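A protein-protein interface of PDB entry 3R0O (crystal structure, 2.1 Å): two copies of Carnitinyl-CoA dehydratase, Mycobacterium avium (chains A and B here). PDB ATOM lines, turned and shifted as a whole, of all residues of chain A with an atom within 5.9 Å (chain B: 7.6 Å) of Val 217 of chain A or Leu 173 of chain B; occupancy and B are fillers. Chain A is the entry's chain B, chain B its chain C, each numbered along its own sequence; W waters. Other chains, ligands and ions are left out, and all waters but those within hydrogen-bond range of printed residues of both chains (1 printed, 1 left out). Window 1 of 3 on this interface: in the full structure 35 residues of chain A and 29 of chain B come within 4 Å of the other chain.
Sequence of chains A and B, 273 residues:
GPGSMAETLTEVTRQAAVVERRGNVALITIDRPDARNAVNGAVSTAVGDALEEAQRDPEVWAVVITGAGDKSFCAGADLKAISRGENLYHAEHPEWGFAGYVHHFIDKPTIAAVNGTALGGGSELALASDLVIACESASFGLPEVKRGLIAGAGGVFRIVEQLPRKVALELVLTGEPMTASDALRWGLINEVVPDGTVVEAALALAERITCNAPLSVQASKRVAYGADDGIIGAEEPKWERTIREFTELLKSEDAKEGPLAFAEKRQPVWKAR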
ATOM      1  N   TRP A  61      -6.893 -33.382  10.977  1.00  0.00           N
ATOM      2  CA  TRP A  61      -7.407 -32.068  11.403  1.00  0.00           C
ATOM      3  C   TRP A  61      -8.124 -32.074  12.735  1.00  0.00           C
ATOM      4  O   TRP A  61      -8.458 -30.999  13.292  1.00  0.00           O
ATOM      5  CB  TRP A  61      -8.307 -31.455  10.339  1.00  0.00           C
ATOM      6  CG  TRP A  61      -7.575 -31.197   9.046  1.00  0.00           C
ATOM      7  CD1 TRP A  61      -6.219 -31.214   8.834  1.00  0.00           C
ATOM      8  CD2 TRP A  61      -8.176 -30.873   7.805  1.00  0.00           C
ATOM      9  NE1 TRP A  61      -5.948 -30.918   7.519  1.00  0.00           N
ATOM     10  CE2 TRP A  61      -7.136 -30.709   6.865  1.00  0.00           C
ATOM     11  CE3 TRP A  61      -9.504 -30.696   7.392  1.00  0.00           C
ATOM     12  CZ2 TRP A  61      -7.383 -30.392   5.523  1.00  0.00           C
ATOM     13  CZ3 TRP A  61      -9.753 -30.378   6.050  1.00  0.00           C
ATOM     14  CH2 TRP A  61      -8.695 -30.229   5.136  1.00  0.00           C
ATOM     15  N   ASP A 107      -1.211 -29.409  18.021  1.00  0.00           N
ATOM     16  CA  ASP A 107      -1.971 -28.395  17.306  1.00  0.00           C
ATOM     17  C   ASP A 107      -3.394 -28.840  16.977  1.00  0.00           C
ATOM     18  O   ASP A 107      -4.265 -27.991  16.804  1.00  0.00           O
ATOM     19  CB  ASP A 107      -1.271 -28.062  15.958  1.00  0.00           C
ATOM     20  CG  ASP A 107       0.077 -27.385  16.154  1.00  0.00           C
ATOM     21  OD1 ASP A 107       0.187 -26.525  17.052  1.00  0.00           O
ATOM     22  OD2 ASP A 107       1.020 -27.713  15.405  1.00  0.00           O
ATOM     23  N   PRO A 109      -7.165 -30.261  17.294  1.00  0.00           N
ATOM     24  CA  PRO A 109      -8.160 -30.406  18.372  1.00  0.00           C
ATOM     25  C   PRO A 109      -8.386 -31.876  18.781  1.00  0.00           C
ATOM     26  O   PRO A 109      -8.408 -32.784  17.932  1.00  0.00           O
ATOM     27  CB  PRO A 109      -9.448 -29.804  17.782  1.00  0.00           C
ATOM     28  CG  PRO A 109      -9.052 -29.074  16.555  1.00  0.00           C
ATOM     29  CD  PRO A 109      -7.664 -29.517  16.124  1.00  0.00           C
ATOM     30  N   ASP A 130      -9.471 -31.060  24.538  1.00  0.00           N
ATOM     31  CA  ASP A 130     -10.155 -29.783  24.220  1.00  0.00           C
ATOM     32  C   ASP A 130     -11.662 -29.789  24.389  1.00  0.00           C
ATOM     33  O   ASP A 130     -12.238 -28.803  24.867  1.00  0.00           O
ATOM     34  CB  ASP A 130      -9.810 -29.349  22.797  1.00  0.00           C
ATOM     35  CG  ASP A 130      -8.325 -29.275  22.590  1.00  0.00           C
ATOM     36  OD1 ASP A 130      -7.653 -28.736  23.485  1.00  0.00           O
ATOM     37  OD2 ASP A 130      -7.822 -29.793  21.588  1.00  0.00           O
ATOM     38  N   LEU A 131     -12.287 -30.908  24.024  1.00  0.00           N
ATOM     39  CA  LEU A 131     -13.751 -31.049  24.068  1.00  0.00           C
ATOM     40  C   LEU A 131     -14.117 -32.422  24.633  1.00  0.00           C
ATOM     41  O   LEU A 131     -13.311 -33.346  24.568  1.00  0.00           O
ATOM     42  CB  LEU A 131     -14.330 -30.891  22.654  1.00  0.00           C
ATOM     43  CG  LEU A 131     -13.977 -29.548  21.947  1.00  0.00           C
ATOM     44  CD1 LEU A 131     -14.191 -29.600  20.457  1.00  0.00           C
ATOM     45  CD2 LEU A 131     -14.724 -28.341  22.524  1.00  0.00           C
ATOM     46  N   ARG A 208     -17.782 -30.799  12.594  1.00  0.00           N
ATOM     47  CA  ARG A 208     -18.122 -29.376  12.749  1.00  0.00           C
ATOM     48  C   ARG A 208     -16.874 -28.542  12.973  1.00  0.00           C
ATOM     49  O   ARG A 208     -16.952 -27.310  13.039  1.00  0.00           O
ATOM     50  CB  ARG A 208     -19.135 -29.169  13.878  1.00  0.00           C
ATOM     51  CG  ARG A 208     -20.542 -29.671  13.505  1.00  0.00           C
ATOM     52  CD  ARG A 208     -21.378 -29.988  14.751  1.00  0.00           C
ATOM     53  NE  ARG A 208     -21.325 -28.919  15.737  1.00  0.00           N
ATOM     54  CZ  ARG A 208     -21.423 -29.088  17.055  1.00  0.00           C
ATOM     55  NH1 ARG A 208     -21.586 -30.297  17.597  1.00  0.00           N
ATOM     56  NH2 ARG A 208     -21.351 -28.027  17.835  1.00  0.00           N
ATOM     57  N   ILE A 209     -15.721 -29.212  13.039  1.00  0.00           N
ATOM     58  CA  ILE A 209     -14.437 -28.547  13.189  1.00  0.00           C
ATOM     59  C   ILE A 209     -13.548 -28.722  11.938  1.00  0.00           C
ATOM     60  O   ILE A 209     -12.952 -27.750  11.463  1.00  0.00           O
ATOM     61  CB  ILE A 209     -13.700 -29.038  14.455  1.00  0.00           C
ATOM     62  CG1 ILE A 209     -14.487 -28.644  15.713  1.00  0.00           C
ATOM     63  CG2 ILE A 209     -12.255 -28.486  14.495  1.00  0.00           C
ATOM     64  CD1 ILE A 209     -14.004 -29.362  16.949  1.00  0.00           C
ATOM     65  N   ASN A 212     -13.778 -26.399   8.959  1.00  0.00           N
ATOM     66  CA  ASN A 212     -13.152 -25.079   9.091  1.00  0.00           C
ATOM     67  C   ASN A 212     -11.687 -25.100   8.629  1.00  0.00           C
ATOM     68  O   ASN A 212     -11.086 -26.167   8.567  1.00  0.00           O
ATOM     69  CB  ASN A 212     -13.218 -24.600  10.555  1.00  0.00           C
ATOM     70  CG  ASN A 212     -14.647 -24.437  11.056  1.00  0.00           C
ATOM     71  OD1 ASN A 212     -15.560 -24.155  10.283  1.00  0.00           O
ATOM     72  ND2 ASN A 212     -14.845 -24.637  12.342  1.00  0.00           N
ATOM     73  N   ALA A 213     -11.108 -23.927   8.347  1.00  0.00           N
ATOM     74  CA  ALA A 213      -9.700 -23.877   7.884  1.00  0.00           C
ATOM     75  C   ALA A 213      -8.756 -24.490   8.931  1.00  0.00           C
ATOM     76  O   ALA A 213      -8.730 -24.057  10.081  1.00  0.00           O
ATOM     77  CB  ALA A 213      -9.276 -22.452   7.525  1.00  0.00           C
ATOM     78  N   PRO A 214      -8.013 -25.537   8.543  1.00  0.00           N
ATOM     79  CA  PRO A 214      -7.221 -26.280   9.524  1.00  0.00           C
ATOM     80  C   PRO A 214      -6.169 -25.397  10.226  1.00  0.00           C
ATOM     81  O   PRO A 214      -6.024 -25.494  11.437  1.00  0.00           O
ATOM     82  CB  PRO A 214      -6.539 -27.383   8.681  1.00  0.00           C
ATOM     83  CG  PRO A 214      -6.706 -26.943   7.241  1.00  0.00           C
ATOM     84  CD  PRO A 214      -8.002 -26.175   7.218  1.00  0.00           C
ATOM     85  N   LEU A 215      -5.466 -24.536   9.477  1.00  0.00           N
ATOM     86  CA  LEU A 215      -4.496 -23.639  10.096  1.00  0.00           C
ATOM     87  C   LEU A 215      -5.118 -22.658  11.087  1.00  0.00           C
ATOM     88  O   LEU A 215      -4.466 -22.311  12.074  1.00  0.00           O
ATOM     89  CB  LEU A 215      -3.663 -22.876   9.045  1.00  0.00           C
ATOM     90  CG  LEU A 215      -2.835 -23.715   8.086  1.00  0.00           C
ATOM     91  CD1 LEU A 215      -1.997 -22.781   7.159  1.00  0.00           C
ATOM     92  CD2 LEU A 215      -1.936 -24.711   8.850  1.00  0.00           C
ATOM     93  N   SER A 216      -6.362 -22.218  10.822  1.00  0.00           N
ATOM     94  CA  SER A 216      -7.107 -21.297  11.720  1.00  0.00           C
ATOM     95  C   SER A 216      -7.476 -21.961  13.044  1.00  0.00           C
ATOM     96  O   SER A 216      -7.345 -21.387  14.143  1.00  0.00           O
ATOM     97  CB  SER A 216      -8.428 -20.873  11.080  1.00  0.00           C
ATOM     98  OG  SER A 216      -8.220 -20.076   9.941  1.00  0.00           O
ATOM     99  N   VAL A 217      -8.062 -23.144  12.900  1.00  0.00           N
ATOM    100  CA  VAL A 217      -8.463 -23.957  14.032  1.00  0.00           C
ATOM    101  C   VAL A 217      -7.236 -24.186  14.928  1.00  0.00           C
ATOM    102  O   VAL A 217      -7.308 -23.991  16.120  1.00  0.00           O
ATOM    103  CB  VAL A 217      -9.048 -25.276  13.543  1.00  0.00           C
ATOM    104  CG1 VAL A 217      -9.227 -26.270  14.691  1.00  0.00           C
ATOM    105  CG2 VAL A 217     -10.387 -25.004  12.851  1.00  0.00           C
ATOM    106  N   GLN A 218      -6.118 -24.593  14.335  1.00  0.00           N
ATOM    107  CA  GLN A 218      -4.926 -24.933  15.110  1.00  0.00           C
ATOM    108  C   GLN A 218      -4.249 -23.708  15.773  1.00  0.00           C
ATOM    109  O   GLN A 218      -3.821 -23.774  16.934  1.00  0.00           O
ATOM    110  CB  GLN A 218      -3.956 -25.702  14.212  1.00  0.00           C
ATOM    111  CG  GLN A 218      -4.575 -27.014  13.683  1.00  0.00           C
ATOM    112  CD  GLN A 218      -3.798 -27.554  12.521  1.00  0.00           C
ATOM    113  OE1 GLN A 218      -2.605 -27.303  12.417  1.00  0.00           O
ATOM    114  NE2 GLN A 218      -4.468 -28.291  11.631  1.00  0.00           N
ATOM    115  N   ALA A 219      -4.164 -22.600  15.041  1.00  0.00           N
ATOM    116  CA  ALA A 219      -3.682 -21.334  15.602  1.00  0.00           C
ATOM    117  C   ALA A 219      -4.603 -20.873  16.736  1.00  0.00           C
ATOM    118  O   ALA A 219      -4.127 -20.377  17.777  1.00  0.00           O
ATOM    119  CB  ALA A 219      -3.591 -20.276  14.510  1.00  0.00           C
ATOM    120  N   SER A 220      -5.914 -21.057  16.561  1.00  0.00           N
ATOM    121  CA  SER A 220      -6.871 -20.675  17.613  1.00  0.00           C
ATOM    122  C   SER A 220      -6.660 -21.496  18.860  1.00  0.00           C
ATOM    123  O   SER A 220      -6.723 -20.963  19.982  1.00  0.00           O
ATOM    124  CB  SER A 220      -8.329 -20.814  17.136  1.00  0.00           C
ATOM    125  OG  SER A 220      -8.606 -19.884  16.106  1.00  0.00           O
ATOM    126  N   LYS A 221      -6.377 -22.787  18.676  1.00  0.00           N
ATOM    127  CA  LYS A 221      -6.056 -23.658  19.804  1.00  0.00           C
ATOM    128  C   LYS A 221      -4.831 -23.155  20.568  1.00  0.00           C
ATOM    129  O   LYS A 221      -4.858 -23.030  21.791  1.00  0.00           O
ATOM    130  CB  LYS A 221      -5.838 -25.114  19.341  1.00  0.00           C
ATOM    131  CG  LYS A 221      -5.581 -26.072  20.532  1.00  0.00           C
ATOM    132  CD  LYS A 221      -5.544 -27.553  20.113  1.00  0.00           C
ATOM    133  CE  LYS A 221      -4.882 -28.412  21.211  1.00  0.00           C
ATOM    134  NZ  LYS A 221      -5.126 -29.873  21.063  1.00  0.00           N
ATOM    135  N   ARG A 222      -3.777 -22.826  19.837  1.00  0.00           N
ATOM    136  CA  ARG A 222      -2.524 -22.295  20.444  1.00  0.00           C
ATOM    137  C   ARG A 222      -2.746 -21.008  21.233  1.00  0.00           C
ATOM    138  O   ARG A 222      -2.302 -20.879  22.379  1.00  0.00           O
ATOM    139  CB  ARG A 222      -1.474 -22.059  19.362  1.00  0.00           C
ATOM    140  CG  ARG A 222      -0.872 -23.362  18.844  1.00  0.00           C
ATOM    141  CD  ARG A 222       0.385 -23.126  18.003  1.00  0.00           C
ATOM    142  NE  ARG A 222       0.135 -22.321  16.804  1.00  0.00           N
ATOM    143  CZ  ARG A 222      -0.210 -22.801  15.610  1.00  0.00           C
ATOM    144  NH1 ARG A 222      -0.375 -24.110  15.426  1.00  0.00           N
ATOM    145  NH2 ARG A 222      -0.353 -21.967  14.580  1.00  0.00           N
ATOM    146  N   LEU B 142     -17.296 -16.306  16.984  1.00  0.00           N
ATOM    147  CA  LEU B 142     -16.048 -15.961  16.309  1.00  0.00           C
ATOM    148  C   LEU B 142     -15.905 -16.875  15.092  1.00  0.00           C
ATOM    149  O   LEU B 142     -15.176 -17.869  15.130  1.00  0.00           O
ATOM    150  CB  LEU B 142     -14.867 -16.110  17.273  1.00  0.00           C
ATOM    151  CG  LEU B 142     -15.000 -15.374  18.616  1.00  0.00           C
ATOM    152  CD1 LEU B 142     -13.897 -15.840  19.569  1.00  0.00           C
ATOM    153  CD2 LEU B 142     -14.936 -13.840  18.396  1.00  0.00           C
ATOM    154  N   GLU B 144     -14.375 -16.477  12.306  1.00  0.00           N
ATOM    155  CA  GLU B 144     -13.157 -16.313  11.493  1.00  0.00           C
ATOM    156  C   GLU B 144     -12.526 -17.662  11.063  1.00  0.00           C
ATOM    157  O   GLU B 144     -11.988 -17.775   9.966  1.00  0.00           O
ATOM    158  CB  GLU B 144     -12.100 -15.478  12.256  1.00  0.00           C
ATOM    159  CG  GLU B 144     -12.429 -13.979  12.452  1.00  0.00           C
ATOM    160  CD  GLU B 144     -13.234 -13.650  13.748  1.00  0.00           C
ATOM    161  OE1 GLU B 144     -13.836 -14.569  14.348  1.00  0.00           O
ATOM    162  OE2 GLU B 144     -13.255 -12.448  14.169  1.00  0.00           O
ATOM    163  N   VAL B 145     -12.592 -18.678  11.918  1.00  0.00           N
ATOM    164  CA  VAL B 145     -12.037 -19.997  11.586  1.00  0.00           C
ATOM    165  C   VAL B 145     -12.642 -20.611  10.330  1.00  0.00           C
ATOM    166  O   VAL B 145     -12.046 -21.496   9.711  1.00  0.00           O
ATOM    167  CB  VAL B 145     -12.169 -21.015  12.767  1.00  0.00           C
ATOM    168  CG1 VAL B 145     -11.276 -20.590  13.911  1.00  0.00           C
ATOM    169  CG2 VAL B 145     -13.633 -21.151  13.226  1.00  0.00           C
ATOM    170  N   LYS B 146     -13.833 -20.157   9.956  1.00  0.00           N
ATOM    171  CA  LYS B 146     -14.459 -20.660   8.746  1.00  0.00           C
ATOM    172  C   LYS B 146     -13.885 -19.995   7.485  1.00  0.00           C
ATOM    173  O   LYS B 146     -14.142 -20.454   6.379  1.00  0.00           O
ATOM    174  CB  LYS B 146     -15.994 -20.528   8.807  1.00  0.00           C
ATOM    175  CG  LYS B 146     -16.631 -21.296   9.986  1.00  0.00           C
ATOM    176  CD  LYS B 146     -18.161 -21.258   9.975  1.00  0.00           C
ATOM    177  CE  LYS B 146     -18.723 -22.237  11.004  1.00  0.00           C
ATOM    178  NZ  LYS B 146     -18.357 -23.656  10.728  1.00  0.00           N
ATOM    179  N   GLY B 148     -10.382 -18.849   7.221  1.00  0.00           N
ATOM    180  CA  GLY B 148      -8.926 -18.922   7.088  1.00  0.00           C
ATOM    181  C   GLY B 148      -8.128 -18.012   8.016  1.00  0.00           C
ATOM    182  O   GLY B 148      -6.906 -18.030   7.975  1.00  0.00           O
ATOM    183  N   LEU B 149      -8.789 -17.219   8.860  1.00  0.00           N
ATOM    184  CA  LEU B 149      -8.066 -16.334   9.801  1.00  0.00           C
ATOM    185  C   LEU B 149      -8.481 -16.688  11.227  1.00  0.00           C
ATOM    186  O   LEU B 149      -9.133 -17.712  11.424  1.00  0.00           O
ATOM    187  CB  LEU B 149      -8.330 -14.853   9.484  1.00  0.00           C
ATOM    188  CG  LEU B 149      -7.857 -14.368   8.096  1.00  0.00           C
ATOM    189  CD1 LEU B 149      -8.224 -12.889   7.843  1.00  0.00           C
ATOM    190  CD2 LEU B 149      -6.345 -14.611   7.893  1.00  0.00           C
ATOM    191  N   ILE B 150      -8.094 -15.882  12.210  1.00  0.00           N
ATOM    192  CA  ILE B 150      -8.563 -16.059  13.584  1.00  0.00           C
ATOM    193  C   ILE B 150      -9.171 -14.745  14.089  1.00  0.00           C
ATOM    194  O   ILE B 150      -9.005 -13.708  13.443  1.00  0.00           O
ATOM    195  CB  ILE B 150      -7.446 -16.484  14.577  1.00  0.00           C
ATOM    196  CG1 ILE B 150      -6.282 -15.499  14.592  1.00  0.00           C
ATOM    197  CG2 ILE B 150      -6.970 -17.926  14.323  1.00  0.00           C
ATOM    198  CD1 ILE B 150      -5.297 -15.813  15.739  1.00  0.00           C
ATOM    199  N   VAL B 156     -10.164 -14.774  20.928  1.00  0.00           N
ATOM    200  CA  VAL B 156      -9.761 -16.143  21.339  1.00  0.00           C
ATOM    201  C   VAL B 156      -9.333 -16.212  22.805  1.00  0.00           C
ATOM    202  O   VAL B 156      -9.855 -17.046  23.569  1.00  0.00           O
ATOM    203  CB  VAL B 156      -8.684 -16.755  20.434  1.00  0.00           C
ATOM    204  CG1 VAL B 156      -8.371 -18.234  20.845  1.00  0.00           C
ATOM    205  CG2 VAL B 156      -9.116 -16.680  18.963  1.00  0.00           C
ATOM    206  N   LYS B 166     -14.467 -25.533  28.329  1.00  0.00           N
ATOM    207  CA  LYS B 166     -14.889 -26.472  27.277  1.00  0.00           C
ATOM    208  C   LYS B 166     -15.908 -25.792  26.350  1.00  0.00           C
ATOM    209  O   LYS B 166     -15.926 -26.027  25.137  1.00  0.00           O
ATOM    210  CB  LYS B 166     -15.488 -27.762  27.860  1.00  0.00           C
ATOM    211  CG  LYS B 166     -14.603 -28.992  27.728  1.00  0.00           C
ATOM    212  CD  LYS B 166     -13.307 -28.855  28.505  1.00  0.00           C
ATOM    213  CE  LYS B 166     -12.465 -30.096  28.285  1.00  0.00           C
ATOM    214  NZ  LYS B 166     -11.062 -29.911  28.786  1.00  0.00           N
ATOM    215  N   VAL B 167     -16.758 -24.959  26.934  1.00  0.00           N
ATOM    216  CA  VAL B 167     -17.762 -24.247  26.164  1.00  0.00           C
ATOM    217  C   VAL B 167     -17.121 -23.193  25.244  1.00  0.00           C
ATOM    218  O   VAL B 167     -17.541 -23.055  24.079  1.00  0.00           O
ATOM    219  CB  VAL B 167     -18.809 -23.616  27.077  1.00  0.00           C
ATOM    220  CG1 VAL B 167     -19.800 -22.746  26.269  1.00  0.00           C
ATOM    221  CG2 VAL B 167     -19.531 -24.720  27.846  1.00  0.00           C
ATOM    222  N   ALA B 168     -16.144 -22.444  25.770  1.00  0.00           N
ATOM    223  CA  ALA B 168     -15.361 -21.488  24.962  1.00  0.00           C
ATOM    224  C   ALA B 168     -14.663 -22.205  23.825  1.00  0.00           C
ATOM    225  O   ALA B 168     -14.647 -21.708  22.686  1.00  0.00           O
ATOM    226  CB  ALA B 168     -14.297 -20.740  25.837  1.00  0.00           C
ATOM    227  N   LEU B 169     -14.068 -23.364  24.116  1.00  0.00           N
ATOM    228  CA  LEU B 169     -13.294 -24.050  23.090  1.00  0.00           C
ATOM    229  C   LEU B 169     -14.189 -24.523  21.944  1.00  0.00           C
ATOM    230  O   LEU B 169     -13.830 -24.423  20.766  1.00  0.00           O
ATOM    231  CB  LEU B 169     -12.397 -25.162  23.677  1.00  0.00           C
ATOM    232  CG  LEU B 169     -11.063 -24.562  24.159  1.00  0.00           C
ATOM    233  CD1 LEU B 169     -10.446 -25.470  25.109  1.00  0.00           C
ATOM    234  CD2 LEU B 169     -10.101 -24.281  22.978  1.00  0.00           C
ATOM    235  N   GLU B 170     -15.378 -24.991  22.285  1.00  0.00           N
ATOM    236  CA  GLU B 170     -16.335 -25.379  21.249  1.00  0.00           C
ATOM    237  C   GLU B 170     -16.677 -24.170  20.370  1.00  0.00           C
ATOM    238  O   GLU B 170     -16.718 -24.273  19.139  1.00  0.00           O
ATOM    239  CB  GLU B 170     -17.575 -26.019  21.882  1.00  0.00           C
ATOM    240  CG  GLU B 170     -18.708 -26.262  20.900  1.00  0.00           C
ATOM    241  CD  GLU B 170     -19.922 -26.881  21.561  1.00  0.00           C
ATOM    242  OE1 GLU B 170     -19.830 -27.309  22.746  1.00  0.00           O
ATOM    243  OE2 GLU B 170     -20.969 -26.962  20.877  1.00  0.00           O
ATOM    244  N   LEU B 171     -16.916 -23.022  20.995  1.00  0.00           N
ATOM    245  CA  LEU B 171     -17.253 -21.825  20.218  1.00  0.00           C
ATOM    246  C   LEU B 171     -16.084 -21.424  19.311  1.00  0.00           C
ATOM    247  O   LEU B 171     -16.284 -21.087  18.118  1.00  0.00           O
ATOM    248  CB  LEU B 171     -17.632 -20.669  21.154  1.00  0.00           C
ATOM    249  CG  LEU B 171     -18.056 -19.325  20.558  1.00  0.00           C
ATOM    250  CD1 LEU B 171     -19.071 -18.635  21.483  1.00  0.00           C
ATOM    251  CD2 LEU B 171     -16.840 -18.415  20.229  1.00  0.00           C
ATOM    252  N   VAL B 172     -14.868 -21.457  19.867  1.00  0.00           N
ATOM    253  CA  VAL B 172     -13.694 -21.060  19.119  1.00  0.00           C
ATOM    254  C   VAL B 172     -13.365 -21.989  17.937  1.00  0.00           C
ATOM    255  O   VAL B 172     -13.057 -21.519  16.839  1.00  0.00           O
ATOM    256  CB  VAL B 172     -12.455 -20.924  20.043  1.00  0.00           C
ATOM    257  CG1 VAL B 172     -11.184 -20.827  19.233  1.00  0.00           C
ATOM    258  CG2 VAL B 172     -12.619 -19.731  20.964  1.00  0.00           C
ATOM    259  N   LEU B 173     -13.414 -23.298  18.176  1.00  0.00           N
ATOM    260  CA  LEU B 173     -12.959 -24.287  17.198  1.00  0.00           C
ATOM    261  C   LEU B 173     -14.027 -24.570  16.134  1.00  0.00           C
ATOM    262  O   LEU B 173     -13.688 -24.904  15.031  1.00  0.00           O
ATOM    263  CB  LEU B 173     -12.552 -25.592  17.898  1.00  0.00           C
ATOM    264  CG  LEU B 173     -11.485 -25.477  19.010  1.00  0.00           C
ATOM    265  CD1 LEU B 173     -11.248 -26.819  19.721  1.00  0.00           C
ATOM    266  CD2 LEU B 173     -10.157 -24.905  18.488  1.00  0.00           C
ATOM    267  N   THR B 174     -15.315 -24.457  16.475  1.00  0.00           N
ATOM    268  CA  THR B 174     -16.372 -24.679  15.492  1.00  0.00           C
ATOM    269  C   THR B 174     -16.705 -23.415  14.708  1.00  0.00           C
ATOM    270  O   THR B 174     -17.176 -23.487  13.564  1.00  0.00           O
ATOM    271  CB  THR B 174     -17.679 -25.220  16.111  1.00  0.00           C
ATOM    272  OG1 THR B 174     -18.262 -24.208  16.944  1.00  0.00           O
ATOM    273  CG2 THR B 174     -17.445 -26.491  16.918  1.00  0.00           C
ATOM    274  N   GLY B 175     -16.471 -22.261  15.318  1.00  0.00           N
ATOM    275  CA  GLY B 175     -16.879 -20.987  14.724  1.00  0.00           C
ATOM    276  C   GLY B 175     -18.392 -20.768  14.686  1.00  0.00           C
ATOM    277  O   GLY B 175     -18.867 -19.889  13.967  1.00  0.00           O
ATOM    278  N   GLU B 176     -19.140 -21.551  15.463  1.00  0.00           N
ATOM    279  CA  GLU B 176     -20.618 -21.500  15.496  1.00  0.00           C
ATOM    280  C   GLU B 176     -21.157 -20.433  16.485  1.00  0.00           C
ATOM    281  O   GLU B 176     -20.485 -20.102  17.478  1.00  0.00           O
ATOM    282  CB  GLU B 176     -21.171 -22.889  15.849  1.00  0.00           C
ATOM    283  CG  GLU B 176     -21.179 -23.902  14.700  1.00  0.00           C
ATOM    284  CD  GLU B 176     -21.343 -25.350  15.190  1.00  0.00           C
ATOM    285  OE1 GLU B 176     -21.797 -25.575  16.343  1.00  0.00           O
ATOM    286  OE2 GLU B 176     -20.991 -26.278  14.446  1.00  0.00           O
ATOM    287  N   LEU B 249      -1.262 -16.450   9.403  1.00  0.00           N
ATOM    288  CA  LEU B 249      -2.445 -16.884   8.663  1.00  0.00           C
ATOM    289  C   LEU B 249      -2.752 -16.000   7.444  1.00  0.00           C
ATOM    290  O   LEU B 249      -3.106 -16.530   6.383  1.00  0.00           O
ATOM    291  CB  LEU B 249      -3.684 -17.005   9.568  1.00  0.00           C
ATOM    292  CG  LEU B 249      -3.613 -17.998  10.745  1.00  0.00           C
ATOM    293  CD1 LEU B 249      -4.757 -17.752  11.702  1.00  0.00           C
ATOM    294  CD2 LEU B 249      -3.607 -19.430  10.251  1.00  0.00           C
HETATM  295  O   HOH W   1     -10.716 -27.436  27.026  1.00  0.00           O
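NH2 of Arg 208 of chain A is in salt-bridge range of OE1 of Glu 176 of chain B (2.9 Å).
N of Ala 213 of chain A lies within hydrogen-bond range of O of Val 145 of chain B (2.9 Å).
NH2 of Arg 208 of chain A lies within salt-bridge range of OE2 of Glu 170 of chain B, at 3.2 Å.
OD1 of Asn 212 of chain A is in hydrogen-bond range of NZ of Lys 146 of chain B.
OG of Ser 216 of chain A lies close to O of Gly 148 of chain B, 3.1 Å away.
The backbone carbonyl oxygen of Thr 174 of chain B sits at hydrogen-bond distance from the side-chain amide nitrogen of Asn 212 of chain A, at 2.9 Å.
ND2 of Asn 212 of chain A is in hydrogen-bond range of O of Leu 173 of chain B.
The side-chain hydroxyl (OG) of Ser 216 of chain A sits at hydrogen-bond distance from the backbone carbonyl oxygen (O) of Leu 149 of chain B (2.9 Å).
The side-chain carboxylate (OD2) of Asp 130 of chain A lies within salt-bridge range of the side-chain amino group (NZ) of Lys 221 of chain A (2.7 Å).
The side-chain amino group (NZ) of Lys 146 of chain B sits at hydrogen-bond distance from the backbone carbonyl oxygen (O) of Thr 174 of chain B.
The side-chain hydroxyl (OG1) of Thr 174 of chain B lies close to the backbone NH (N) of Glu 176 of chain B, at 3.2 Å.
Among the printed residues, pairs that only touch across the chains: Pro 109 of chain A with Leu 173 of chain B, Asp 130 of chain A with Lys 166 of chain B, Asp 130 of chain A with Leu 169 of chain B, Leu 131 of chain A with Lys 166 of chain B, Leu 131 of chain A with Leu 169 of chain B, Leu 131 of chain A with Glu 170 of chain B, Arg 208 of chain A with Thr 174 of chain B, Ile 209 of chain A with Leu 173 of chain B, Ile 209 of chain A with Thr 174 of chain B, Asn 212 of chain A with Val 145 of chain B, Ala 213 of chain A with Gly 148 of chain B, Leu 215 of chain A with Leu 249 of chain B, Ser 216 of chain A with Val 145 of chain B, Ser 216 of chain A with Ile 150 of chain B, Ser 216 of chain A with Leu 249 of chain B, Val 217 of chain A with Leu 173 of chain B, Ala 219 of chain A with Leu 249 of chain B, Ser 220 of chain A with Val 145 of chain B, Ser 220 of chain A with Ile 150 of chain B, Ser 220 of chain A with Val 156 of chain B and Ser 220 of chain A with Val 172 of chain B.
Of the printed residues of chain B, Pro 109 of chain A touches Leu 173.
Val 217 of chain A touches one residue of chain B.
Of the printed residues of chain B, Ser 220 of chain A touches Val 145, Ile 150, Val 156 and Val 172.
Of the printed residues of chain A, Val 145 of chain B touches Asn 212, Ala 213, Ser 216 and Ser 220.
Ala 168 of chain B touches none of the printed residues of chain A.
The nearest residue of chain B that does not touch Val 217 of chain A is Val 145 of chain B (4.2 Å).
Printed residues of chain B that touch a printed residue of chain A: Val 145, Lys 146, Gly 148, Leu 149, Ile 150, Val 156, Lys 166, Leu 169, Glu 170, Val 172, Leu 173, Thr 174, Glu 176 and Leu 249.
Hydrophobic or aromatic side chains of chain B within 4 Å of the printed part of chain A: Val 145, Ile 150, Val 156, Leu 169, Val 172, Leu 173 and Leu 249.
Among the printed residues, 29 pairs touch across the chains.
No position is printed for both chains.
Of the 29 pairs that touch across the chains among the printed residues, none has its exchanged pair printed and touching as well.
Water W1 lies within hydrogen-bond range of O of Asp 130 of chain A (3.0 Å) and NZ of Lys 166 of chain B (3.1 Å).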
